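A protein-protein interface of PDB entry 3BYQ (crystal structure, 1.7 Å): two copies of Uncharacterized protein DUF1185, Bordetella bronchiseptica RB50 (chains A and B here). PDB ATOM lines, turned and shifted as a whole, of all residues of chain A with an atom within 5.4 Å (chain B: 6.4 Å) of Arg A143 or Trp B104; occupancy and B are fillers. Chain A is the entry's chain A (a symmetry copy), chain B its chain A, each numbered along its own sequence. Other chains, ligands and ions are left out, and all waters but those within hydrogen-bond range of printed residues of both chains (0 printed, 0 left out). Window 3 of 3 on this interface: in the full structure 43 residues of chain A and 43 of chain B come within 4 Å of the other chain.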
ATOM      1  N   TYR A 141      -5.750  -0.854 -23.515  1.00  0.00           N
ATOM      2  CA  TYR A 141      -5.169  -2.199 -23.681  1.00  0.00           C
ATOM      3  C   TYR A 141      -5.363  -3.167 -22.525  1.00  0.00           C
ATOM      4  O   TYR A 141      -4.998  -4.354 -22.637  1.00  0.00           O
ATOM      5  CB  TYR A 141      -3.687  -2.118 -24.034  1.00  0.00           C
ATOM      6  CG  TYR A 141      -3.415  -1.787 -25.487  1.00  0.00           C
ATOM      7  CD1 TYR A 141      -3.265  -0.479 -25.918  1.00  0.00           C
ATOM      8  CD2 TYR A 141      -3.303  -2.809 -26.439  1.00  0.00           C
ATOM      9  CE1 TYR A 141      -2.981  -0.191 -27.249  1.00  0.00           C
ATOM     10  CE2 TYR A 141      -3.039  -2.529 -27.765  1.00  0.00           C
ATOM     11  CZ  TYR A 141      -2.884  -1.231 -28.167  1.00  0.00           C
ATOM     12  OH  TYR A 141      -2.632  -0.976 -29.490  1.00  0.00           O
ATOM     13  N   VAL A 142      -5.974  -2.711 -21.433  1.00  0.00           N
ATOM     14  CA  VAL A 142      -6.215  -3.628 -20.289  1.00  0.00           C
ATOM     15  C   VAL A 142      -7.208  -4.722 -20.738  1.00  0.00           C
ATOM     16  O   VAL A 142      -8.447  -4.548 -20.808  1.00  0.00           O
ATOM     17  CB  VAL A 142      -6.661  -2.889 -19.044  1.00  0.00           C
ATOM     18  CG1 VAL A 142      -7.116  -3.848 -17.968  1.00  0.00           C
ATOM     19  CG2 VAL A 142      -5.482  -2.016 -18.577  1.00  0.00           C
ATOM     20  N   ARG A 143      -6.634  -5.902 -20.958  1.00  0.00           N
ATOM     21  CA  ARG A 143      -7.343  -7.002 -21.624  1.00  0.00           C
ATOM     22  C   ARG A 143      -8.520  -7.572 -20.862  1.00  0.00           C
ATOM     23  O   ARG A 143      -9.534  -8.008 -21.459  1.00  0.00           O
ATOM     24  CB  ARG A 143      -6.358  -8.124 -21.999  1.00  0.00           C
ATOM     25  CG  ARG A 143      -6.963  -9.170 -22.927  1.00  0.00           C
ATOM     26  CD  ARG A 143      -5.957 -10.231 -23.297  1.00  0.00           C
ATOM     27  NE  ARG A 143      -4.931  -9.698 -24.193  1.00  0.00           N
ATOM     28  CZ  ARG A 143      -3.791 -10.303 -24.494  1.00  0.00           C
ATOM     29  NH1 ARG A 143      -3.455 -11.453 -23.936  1.00  0.00           N
ATOM     30  NH2 ARG A 143      -2.965  -9.713 -25.329  1.00  0.00           N
ATOM     31  N   SER A 144      -8.410  -7.582 -19.538  1.00  0.00           N
ATOM     32  CA  SER A 144      -9.455  -8.107 -18.681  1.00  0.00           C
ATOM     33  C   SER A 144     -10.793  -7.368 -18.819  1.00  0.00           C
ATOM     34  O   SER A 144     -11.836  -7.891 -18.418  1.00  0.00           O
ATOM     35  CB  SER A 144      -9.003  -8.031 -17.223  1.00  0.00           C
ATOM     36  OG  SER A 144      -8.571  -6.701 -16.884  1.00  0.00           O
ATOM     37  N   HIS A 145     -10.730  -6.130 -19.313  1.00  0.00           N
ATOM     38  CA  HIS A 145     -11.903  -5.218 -19.289  1.00  0.00           C
ATOM     39  C   HIS A 145     -12.736  -5.093 -20.551  1.00  0.00           C
ATOM     40  O   HIS A 145     -13.881  -4.573 -20.504  1.00  0.00           O
ATOM     41  CB  HIS A 145     -11.446  -3.835 -18.792  1.00  0.00           C
ATOM     42  CG  HIS A 145     -11.273  -3.762 -17.317  1.00  0.00           C
ATOM     43  ND1 HIS A 145     -10.482  -4.651 -16.620  1.00  0.00           N
ATOM     44  CD2 HIS A 145     -11.752  -2.883 -16.403  1.00  0.00           C
ATOM     45  CE1 HIS A 145     -10.534  -4.357 -15.333  1.00  0.00           C
ATOM     46  NE2 HIS A 145     -11.271  -3.269 -15.177  1.00  0.00           N
ATOM     47  N   PHE A 146     -12.244  -5.653 -21.643  1.00  0.00           N
ATOM     48  CA  PHE A 146     -12.989  -5.612 -22.904  1.00  0.00           C
ATOM     49  C   PHE A 146     -14.279  -6.338 -22.678  1.00  0.00           C
ATOM     50  O   PHE A 146     -14.279  -7.450 -22.162  1.00  0.00           O
ATOM     51  CB  PHE A 146     -12.257  -6.257 -24.095  1.00  0.00           C
ATOM     52  CG  PHE A 146     -10.942  -5.620 -24.426  1.00  0.00           C
ATOM     53  CD1 PHE A 146     -10.897  -4.294 -24.743  1.00  0.00           C
ATOM     54  CD2 PHE A 146      -9.777  -6.364 -24.460  1.00  0.00           C
ATOM     55  CE1 PHE A 146      -9.691  -3.692 -25.052  1.00  0.00           C
ATOM     56  CE2 PHE A 146      -8.580  -5.775 -24.768  1.00  0.00           C
ATOM     57  CZ  PHE A 146      -8.545  -4.443 -25.058  1.00  0.00           C
ATOM     58  N   ARG A 173     -14.432  -8.530 -17.083  1.00  0.00           N
ATOM     59  CA  ARG A 173     -15.332  -9.635 -17.441  1.00  0.00           C
ATOM     60  C   ARG A 173     -15.353 -10.581 -16.230  1.00  0.00           C
ATOM     61  O   ARG A 173     -14.322 -10.762 -15.570  1.00  0.00           O
ATOM     62  CB  ARG A 173     -14.828 -10.398 -18.650  1.00  0.00           C
ATOM     63  CG  ARG A 173     -14.821  -9.622 -19.975  1.00  0.00           C
ATOM     64  CD  ARG A 173     -14.460 -10.518 -21.178  1.00  0.00           C
ATOM     65  NE  ARG A 173     -13.134 -11.077 -20.991  1.00  0.00           N
ATOM     66  CZ  ARG A 173     -12.002 -10.420 -21.197  1.00  0.00           C
ATOM     67  NH1 ARG A 173     -11.997  -9.170 -21.597  1.00  0.00           N
ATOM     68  NH2 ARG A 173     -10.858 -11.021 -20.956  1.00  0.00           N
ATOM     69  N   LEU A 178      -7.325 -14.110 -19.626  1.00  0.00           N
ATOM     70  CA  LEU A 178      -6.518 -14.151 -20.851  1.00  0.00           C
ATOM     71  C   LEU A 178      -5.236 -13.342 -20.789  1.00  0.00           C
ATOM     72  O   LEU A 178      -4.616 -13.027 -21.805  1.00  0.00           O
ATOM     73  CB  LEU A 178      -7.388 -13.738 -22.045  1.00  0.00           C
ATOM     74  CG  LEU A 178      -8.575 -14.646 -22.414  1.00  0.00           C
ATOM     75  CD1 LEU A 178      -9.332 -13.993 -23.558  1.00  0.00           C
ATOM     76  CD2 LEU A 178      -8.127 -16.062 -22.712  1.00  0.00           C
ATOM     77  N   GLY A 179      -4.842 -12.995 -19.575  1.00  0.00           N
ATOM     78  CA  GLY A 179      -3.608 -12.251 -19.370  1.00  0.00           C
ATOM     79  C   GLY A 179      -3.669 -10.865 -19.964  1.00  0.00           C
ATOM     80  O   GLY A 179      -4.669 -10.185 -19.887  1.00  0.00           O
ATOM     81  N   GLY A 180      -2.579 -10.468 -20.596  1.00  0.00           N
ATOM     82  CA  GLY A 180      -2.488  -9.126 -21.166  1.00  0.00           C
ATOM     83  C   GLY A 180      -2.194  -8.098 -20.099  1.00  0.00           C
ATOM     84  O   GLY A 180      -1.988  -8.424 -18.921  1.00  0.00           O
ATOM     85  N   LEU A 181      -2.187  -6.838 -20.518  1.00  0.00           N
ATOM     86  CA  LEU A 181      -1.933  -5.719 -19.612  1.00  0.00           C
ATOM     87  C   LEU A 181      -2.992  -5.705 -18.534  1.00  0.00           C
ATOM     88  O   LEU A 181      -4.156  -5.789 -18.839  1.00  0.00           O
ATOM     89  CB  LEU A 181      -1.988  -4.403 -20.384  1.00  0.00           C
ATOM     90  CG  LEU A 181      -1.697  -3.127 -19.617  1.00  0.00           C
ATOM     91  CD1 LEU A 181      -0.275  -3.128 -19.051  1.00  0.00           C
ATOM     92  CD2 LEU A 181      -1.918  -1.930 -20.538  1.00  0.00           C
ATOM     93  N   MET B  51      -5.399 -20.236 -23.015  1.00  0.00           N
ATOM     94  CA  MET B  51      -4.153 -19.692 -23.627  1.00  0.00           C
ATOM     95  C   MET B  51      -3.719 -20.431 -24.901  1.00  0.00           C
ATOM     96  O   MET B  51      -3.406 -19.791 -25.905  1.00  0.00           O
ATOM     97  CB  MET B  51      -3.008 -19.537 -22.607  1.00  0.00           C
ATOM     98  CG  MET B  51      -3.383 -18.654 -21.400  1.00  0.00           C
ATOM     99  SD  MET B  51      -3.970 -16.862 -21.805  1.00  0.00           S
ATOM    100  CE  MET B  51      -2.272 -16.040 -22.186  1.00  0.00           C
ATOM    101  N   MET B  54      -6.140 -19.338 -27.656  1.00  0.00           N
ATOM    102  CA  MET B  54      -5.827 -17.962 -28.055  1.00  0.00           C
ATOM    103  C   MET B  54      -4.571 -17.892 -28.941  1.00  0.00           C
ATOM    104  O   MET B  54      -4.499 -17.144 -29.939  1.00  0.00           O
ATOM    105  CB  MET B  54      -5.644 -17.069 -26.835  1.00  0.00           C
ATOM    106  CG  MET B  54      -5.429 -15.620 -27.220  1.00  0.00           C
ATOM    107  SD  MET B  54      -5.642 -14.450 -25.703  1.00  0.00           S
ATOM    108  CE  MET B  54      -3.970 -14.798 -24.849  1.00  0.00           C
ATOM    109  N   ARG B  58      -4.241 -17.140 -33.604  1.00  0.00           N
ATOM    110  CA  ARG B  58      -3.506 -16.150 -34.389  1.00  0.00           C
ATOM    111  C   ARG B  58      -3.440 -16.562 -35.872  1.00  0.00           C
ATOM    112  O   ARG B  58      -3.489 -15.717 -36.792  1.00  0.00           O
ATOM    113  CB  ARG B  58      -2.095 -15.944 -33.804  1.00  0.00           C
ATOM    114  CG  ARG B  58      -1.323 -14.759 -34.337  1.00  0.00           C
ATOM    115  CD  ARG B  58      -1.612 -13.475 -33.600  1.00  0.00           C
ATOM    116  NE  ARG B  58      -1.275 -13.568 -32.176  1.00  0.00           N
ATOM    117  CZ  ARG B  58      -0.059 -13.417 -31.645  1.00  0.00           C
ATOM    118  NH1 ARG B  58       1.001 -13.101 -32.368  1.00  0.00           N
ATOM    119  NH2 ARG B  58       0.087 -13.550 -30.337  1.00  0.00           N
ATOM    120  N   LYS B  82     -12.263  -5.903 -35.577  1.00  0.00           N
ATOM    121  CA  LYS B  82     -12.306  -7.362 -35.299  1.00  0.00           C
ATOM    122  C   LYS B  82     -13.539  -7.666 -34.454  1.00  0.00           C
ATOM    123  O   LYS B  82     -13.983  -6.852 -33.667  1.00  0.00           O
ATOM    124  CB  LYS B  82     -11.012  -7.812 -34.561  1.00  0.00           C
ATOM    125  CG  LYS B  82     -10.826  -7.225 -33.158  1.00  0.00           C
ATOM    126  CD  LYS B  82      -9.398  -7.312 -32.634  1.00  0.00           C
ATOM    127  CE  LYS B  82      -9.228  -6.417 -31.448  1.00  0.00           C
ATOM    128  NZ  LYS B  82      -7.866  -6.398 -30.865  1.00  0.00           N
ATOM    129  N   GLU B  93     -15.674 -15.348 -22.741  1.00  0.00           N
ATOM    130  CA  GLU B  93     -14.209 -15.482 -22.761  1.00  0.00           C
ATOM    131  C   GLU B  93     -13.725 -16.204 -24.018  1.00  0.00           C
ATOM    132  O   GLU B  93     -12.594 -16.007 -24.460  1.00  0.00           O
ATOM    133  CB  GLU B  93     -13.677 -16.211 -21.530  1.00  0.00           C
ATOM    134  CG  GLU B  93     -12.270 -15.766 -21.168  1.00  0.00           C
ATOM    135  CD  GLU B  93     -12.181 -14.345 -20.619  1.00  0.00           C
ATOM    136  OE1 GLU B  93     -13.221 -13.727 -20.355  1.00  0.00           O
ATOM    137  OE2 GLU B  93     -11.048 -13.842 -20.391  1.00  0.00           O
ATOM    138  N   ALA B  96     -13.341 -13.503 -26.365  1.00  0.00           N
ATOM    139  CA  ALA B  96     -12.306 -12.545 -25.898  1.00  0.00           C
ATOM    140  C   ALA B  96     -10.907 -12.907 -26.377  1.00  0.00           C
ATOM    141  O   ALA B  96     -10.020 -12.081 -26.454  1.00  0.00           O
ATOM    142  CB  ALA B  96     -12.341 -12.378 -24.370  1.00  0.00           C
ATOM    143  N   TRP B  98     -10.027 -13.401 -29.201  1.00  0.00           N
ATOM    144  CA  TRP B  98      -9.848 -12.790 -30.524  1.00  0.00           C
ATOM    145  C   TRP B  98      -9.239 -11.383 -30.476  1.00  0.00           C
ATOM    146  O   TRP B  98      -8.744 -10.909 -31.495  1.00  0.00           O
ATOM    147  CB  TRP B  98     -11.177 -12.787 -31.249  1.00  0.00           C
ATOM    148  CG  TRP B  98     -11.117 -12.544 -32.742  1.00  0.00           C
ATOM    149  CD1 TRP B  98     -11.731 -11.524 -33.444  1.00  0.00           C
ATOM    150  CD2 TRP B  98     -10.467 -13.360 -33.715  1.00  0.00           C
ATOM    151  NE1 TRP B  98     -11.462 -11.642 -34.770  1.00  0.00           N
ATOM    152  CE2 TRP B  98     -10.711 -12.778 -34.974  1.00  0.00           C
ATOM    153  CE3 TRP B  98      -9.708 -14.543 -33.642  1.00  0.00           C
ATOM    154  CZ2 TRP B  98     -10.256 -13.353 -36.163  1.00  0.00           C
ATOM    155  CZ3 TRP B  98      -9.244 -15.113 -34.822  1.00  0.00           C
ATOM    156  CH2 TRP B  98      -9.488 -14.490 -36.065  1.00  0.00           C
ATOM    157  N   HIS B  99      -9.245 -10.742 -29.312  1.00  0.00           N
ATOM    158  CA  HIS B  99      -8.635  -9.407 -29.199  1.00  0.00           C
ATOM    159  C   HIS B  99      -7.169  -9.504 -29.615  1.00  0.00           C
ATOM    160  O   HIS B  99      -6.681  -8.759 -30.486  1.00  0.00           O
ATOM    161  CB  HIS B  99      -8.784  -8.804 -27.795  1.00  0.00           C
ATOM    162  CG  HIS B  99     -10.190  -8.408 -27.467  1.00  0.00           C
ATOM    163  ND1 HIS B  99     -10.756  -7.237 -27.918  1.00  0.00           N
ATOM    164  CD2 HIS B  99     -11.145  -9.037 -26.746  1.00  0.00           C
ATOM    165  CE1 HIS B  99     -11.998  -7.152 -27.469  1.00  0.00           C
ATOM    166  NE2 HIS B  99     -12.269  -8.240 -26.763  1.00  0.00           N
ATOM    167  N   GLU B 100      -6.478 -10.463 -29.009  1.00  0.00           N
ATOM    168  CA  GLU B 100      -5.086 -10.698 -29.358  1.00  0.00           C
ATOM    169  C   GLU B 100      -4.969 -11.430 -30.704  1.00  0.00           C
ATOM    170  O   GLU B 100      -4.241 -11.018 -31.597  1.00  0.00           O
ATOM    171  CB  GLU B 100      -4.394 -11.553 -28.305  1.00  0.00           C
ATOM    172  CG  GLU B 100      -2.907 -11.558 -28.504  1.00  0.00           C
ATOM    173  CD  GLU B 100      -2.176 -12.545 -27.637  1.00  0.00           C
ATOM    174  OE1 GLU B 100      -1.749 -12.158 -26.539  1.00  0.00           O
ATOM    175  OE2 GLU B 100      -2.038 -13.702 -28.049  1.00  0.00           O
ATOM    176  N   ALA B 101      -5.691 -12.532 -30.844  1.00  0.00           N
ATOM    177  CA  ALA B 101      -5.501 -13.410 -32.006  1.00  0.00           C
ATOM    178  C   ALA B 101      -5.812 -12.729 -33.330  1.00  0.00           C
ATOM    179  O   ALA B 101      -5.066 -12.835 -34.302  1.00  0.00           O
ATOM    180  CB  ALA B 101      -6.279 -14.729 -31.844  1.00  0.00           C
ATOM    181  N   GLY B 102      -6.898 -11.982 -33.351  1.00  0.00           N
ATOM    182  CA  GLY B 102      -7.318 -11.309 -34.546  1.00  0.00           C
ATOM    183  C   GLY B 102      -6.543 -10.020 -34.721  1.00  0.00           C
ATOM    184  O   GLY B 102      -6.084  -9.712 -35.809  1.00  0.00           O
ATOM    185  N   GLY B 103      -6.440  -9.253 -33.644  1.00  0.00           N
ATOM    186  CA  GLY B 103      -5.774  -7.953 -33.700  1.00  0.00           C
ATOM    187  C   GLY B 103      -4.315  -8.005 -34.041  1.00  0.00           C
ATOM    188  O   GLY B 103      -3.818  -7.287 -34.920  1.00  0.00           O
ATOM    189  N   TRP B 104      -3.574  -8.820 -33.307  1.00  0.00           N
ATOM    190  CA  TRP B 104      -2.145  -8.904 -33.559  1.00  0.00           C
ATOM    191  C   TRP B 104      -1.840  -9.474 -34.948  1.00  0.00           C
ATOM    192  O   TRP B 104      -0.923  -9.018 -35.642  1.00  0.00           O
ATOM    193  CB  TRP B 104      -1.438  -9.708 -32.456  1.00  0.00           C
ATOM    194  CG  TRP B 104      -1.444  -8.993 -31.111  1.00  0.00           C
ATOM    195  CD1 TRP B 104      -2.292  -7.988 -30.697  1.00  0.00           C
ATOM    196  CD2 TRP B 104      -0.665  -9.340 -29.973  1.00  0.00           C
ATOM    197  NE1 TRP B 104      -2.017  -7.649 -29.398  1.00  0.00           N
ATOM    198  CE2 TRP B 104      -1.030  -8.468 -28.929  1.00  0.00           C
ATOM    199  CE3 TRP B 104       0.335 -10.285 -29.742  1.00  0.00           C
ATOM    200  CZ2 TRP B 104      -0.442  -8.522 -27.673  1.00  0.00           C
ATOM    201  CZ3 TRP B 104       0.938 -10.319 -28.491  1.00  0.00           C
ATOM    202  CH2 TRP B 104       0.545  -9.444 -27.482  1.00  0.00           C
ATOM    203  N   ALA B 105      -2.592 -10.478 -35.351  1.00  0.00           N
ATOM    204  CA  ALA B 105      -2.394 -11.108 -36.651  1.00  0.00           C
ATOM    205  C   ALA B 105      -2.637 -10.103 -37.772  1.00  0.00           C
ATOM    206  O   ALA B 105      -1.879 -10.026 -38.752  1.00  0.00           O
ATOM    207  CB  ALA B 105      -3.318 -12.343 -36.830  1.00  0.00           C
ATOM    208  N   MET B 106      -3.703  -9.317 -37.627  1.00  0.00           N
ATOM    209  CA  MET B 106      -4.055  -8.350 -38.679  1.00  0.00           C
ATOM    210  C   MET B 106      -3.012  -7.249 -38.743  1.00  0.00           C
ATOM    211  O   MET B 106      -2.539  -6.848 -39.809  1.00  0.00           O
ATOM    212  CB  MET B 106      -5.465  -7.784 -38.481  1.00  0.00           C
ATOM    213  CG  MET B 106      -5.791  -6.690 -39.485  1.00  0.00           C
ATOM    214  SD  MET B 106      -7.667  -6.483 -39.705  1.00  0.00           S
ATOM    215  CE  MET B 106      -8.039  -5.985 -37.906  1.00  0.00           C
ATOM    216  N   ARG B 107      -2.602  -6.775 -37.591  1.00  0.00           N
ATOM    217  CA  ARG B 107      -1.600  -5.706 -37.567  1.00  0.00           C
ATOM    218  C   ARG B 107      -0.292  -6.189 -38.194  1.00  0.00           C
ATOM    219  O   ARG B 107       0.389  -5.458 -38.893  1.00  0.00           O
ATOM    220  CB  ARG B 107      -1.413  -5.139 -36.159  1.00  0.00           C
ATOM    221  CG  ARG B 107      -2.643  -4.335 -35.767  1.00  0.00           C
ATOM    222  CD  ARG B 107      -2.648  -3.945 -34.288  1.00  0.00           C
ATOM    223  NE  ARG B 107      -1.694  -2.907 -33.972  1.00  0.00           N
ATOM    224  CZ  ARG B 107      -1.395  -2.525 -32.736  1.00  0.00           C
ATOM    225  NH1 ARG B 107      -1.948  -3.117 -31.687  1.00  0.00           N
ATOM    226  NH2 ARG B 107      -0.507  -1.566 -32.545  1.00  0.00           N
ATOM    227  N   SER B 108       0.028  -7.452 -37.968  1.00  0.00           N
ATOM    228  CA  SER B 108       1.270  -8.023 -38.549  1.00  0.00           C
ATOM    229  C   SER B 108       1.182  -8.074 -40.056  1.00  0.00           C
ATOM    230  O   SER B 108       2.121  -7.733 -40.777  1.00  0.00           O
ATOM    231  CB  SER B 108       1.536  -9.421 -37.996  1.00  0.00           C
ATOM    232  OG  SER B 108       1.894  -9.320 -36.628  1.00  0.00           O
ATOM    233  N   VAL B 109       0.022  -8.489 -40.540  1.00  0.00           N
ATOM    234  CA  VAL B 109      -0.209  -8.568 -41.975  1.00  0.00           C
ATOM    235  C   VAL B 109      -0.044  -7.222 -42.639  1.00  0.00           C
ATOM    236  O   VAL B 109       0.525  -7.138 -43.733  1.00  0.00           O
ATOM    237  CB  VAL B 109      -1.609  -9.146 -42.301  1.00  0.00           C
ATOM    238  CG1 VAL B 109      -2.040  -8.825 -43.715  1.00  0.00           C
ATOM    239  CG2 VAL B 109      -1.608 -10.634 -42.063  1.00  0.00           C
ATOM    240  N   GLU B 112       2.407  -3.604 -39.157  1.00  0.00           N
ATOM    241  CA  GLU B 112       2.385  -3.024 -37.828  1.00  0.00           C
ATOM    242  C   GLU B 112       1.914  -1.562 -37.728  1.00  0.00           C
ATOM    243  O   GLU B 112       2.624  -0.715 -37.143  1.00  0.00           O
ATOM    244  CB  GLU B 112       3.760  -3.227 -37.135  1.00  0.00           C
ATOM    245  CG  GLU B 112       4.252  -4.696 -37.105  1.00  0.00           C
ATOM    246  CD  GLU B 112       3.344  -5.660 -36.357  1.00  0.00           C
ATOM    247  OE1 GLU B 112       2.402  -5.215 -35.663  1.00  0.00           O
ATOM    248  OE2 GLU B 112       3.596  -6.891 -36.430  1.00  0.00           O
ATOM    249  N   VAL B 117      -6.738  -2.180 -32.675  1.00  0.00           N
ATOM    250  CA  VAL B 117      -7.798  -2.567 -33.546  1.00  0.00           C
ATOM    251  C   VAL B 117      -9.055  -2.517 -32.660  1.00  0.00           C
ATOM    252  O   VAL B 117      -9.036  -3.111 -31.569  1.00  0.00           O
ATOM    253  CB  VAL B 117      -7.629  -4.006 -34.109  1.00  0.00           C
ATOM    254  CG1 VAL B 117      -8.841  -4.404 -34.951  1.00  0.00           C
ATOM    255  CG2 VAL B 117      -6.296  -4.125 -34.890  1.00  0.00           C
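The side-chain hydroxyl (OH) of Tyr A141 is in hydrogen-bond range of the guanidinium group (NH1) of Arg B107, at 3.1 Å. The guanidinium group (NH2) of Arg A143 lies within salt-bridge range of the side-chain carboxylate (OE1) of Glu B100 (3.0 Å). The side-chain carboxylate (OE1) of Glu B93 is in salt-bridge range of the guanidinium group (NE) of Arg A173 (2.7 Å).
Met B54 touches Arg A143 (CE to NH1, 3.5 Å). Arg A143 touches Trp B104. Phe A146 touches His B99 (CB to NE2, 3.3 Å). Arg A173 touches Ala B96 (NE to CB, 3.7 Å). O of Leu A178 touches CE of Met B51 (3.8 Å). Leu A178 touches Met B54 (O to CE, 3.6 Å). OE2 of Glu B93 touches CG of Leu A178, 3.3 Å away. Ala B96 touches Leu A178 (C to CD1, 3.4 Å).
No position is printed for both chains. Of the 11 pairs that touch across the chains among the printed residues, none has its exchanged pair printed and touching as well.
Of the printed residues of chain B, Arg A143 touches Met B54 (3.5 Å), Glu B100 (3.0 Å) and Trp B104 (3.6 Å). Of the printed residues of chain B, Arg A173 touches Glu B93 and Ala B96. Printed residues of chain B within 4 Å of Leu A178: Met B51 (3.8 Å), Met B54 (3.6 Å), Glu B93 (3.3 Å) and Ala B96 (3.4 Å). Printed residues of chain A within 4 Å of Ala B96: Arg A173 and Leu A178. Printed residues of chain A within 4 Å of Glu B100: Arg A143. Trp B104 touches just one residue of chain A: Arg A143. The nearest printed residue of chain A that does not touch Trp B104 is Tyr A141 (5.5 Å).
O of Leu A178 lies within hydrogen-bond range of NH1 of Arg A143, at 2.9 Å. The backbone NH of Glu B112 is in hydrogen-bond range of the backbone carbonyl oxygen of Arg B107 (2.8 Å). The backbone carbonyl oxygen (O) of Trp B104 sits at hydrogen-bond distance from the side-chain hydroxyl (OG) of Ser B108 (3.0 Å). O of Phe A146 lies within hydrogen-bond range of NH1 of Arg A173, at 2.9 Å. O of Ser A144 sits at hydrogen-bond distance from N of Arg A173, at 3.0 Å. O of Arg A143 sits at hydrogen-bond distance from NH1 of Arg A173 (2.7 Å).
Printed residues of chain B that touch a printed residue of chain A: Met B51, Met B54, Glu B93, Ala B96, His B99, Glu B100, Trp B104 and Arg B107. Among the printed residues, Asp or Glu carboxylates within 4 Å of a Lys or Arg side-chain nitrogen of the other chain: Arg A143 with Glu B100 (3.0 Å) and Arg A173 with Glu B93 (2.7 Å).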
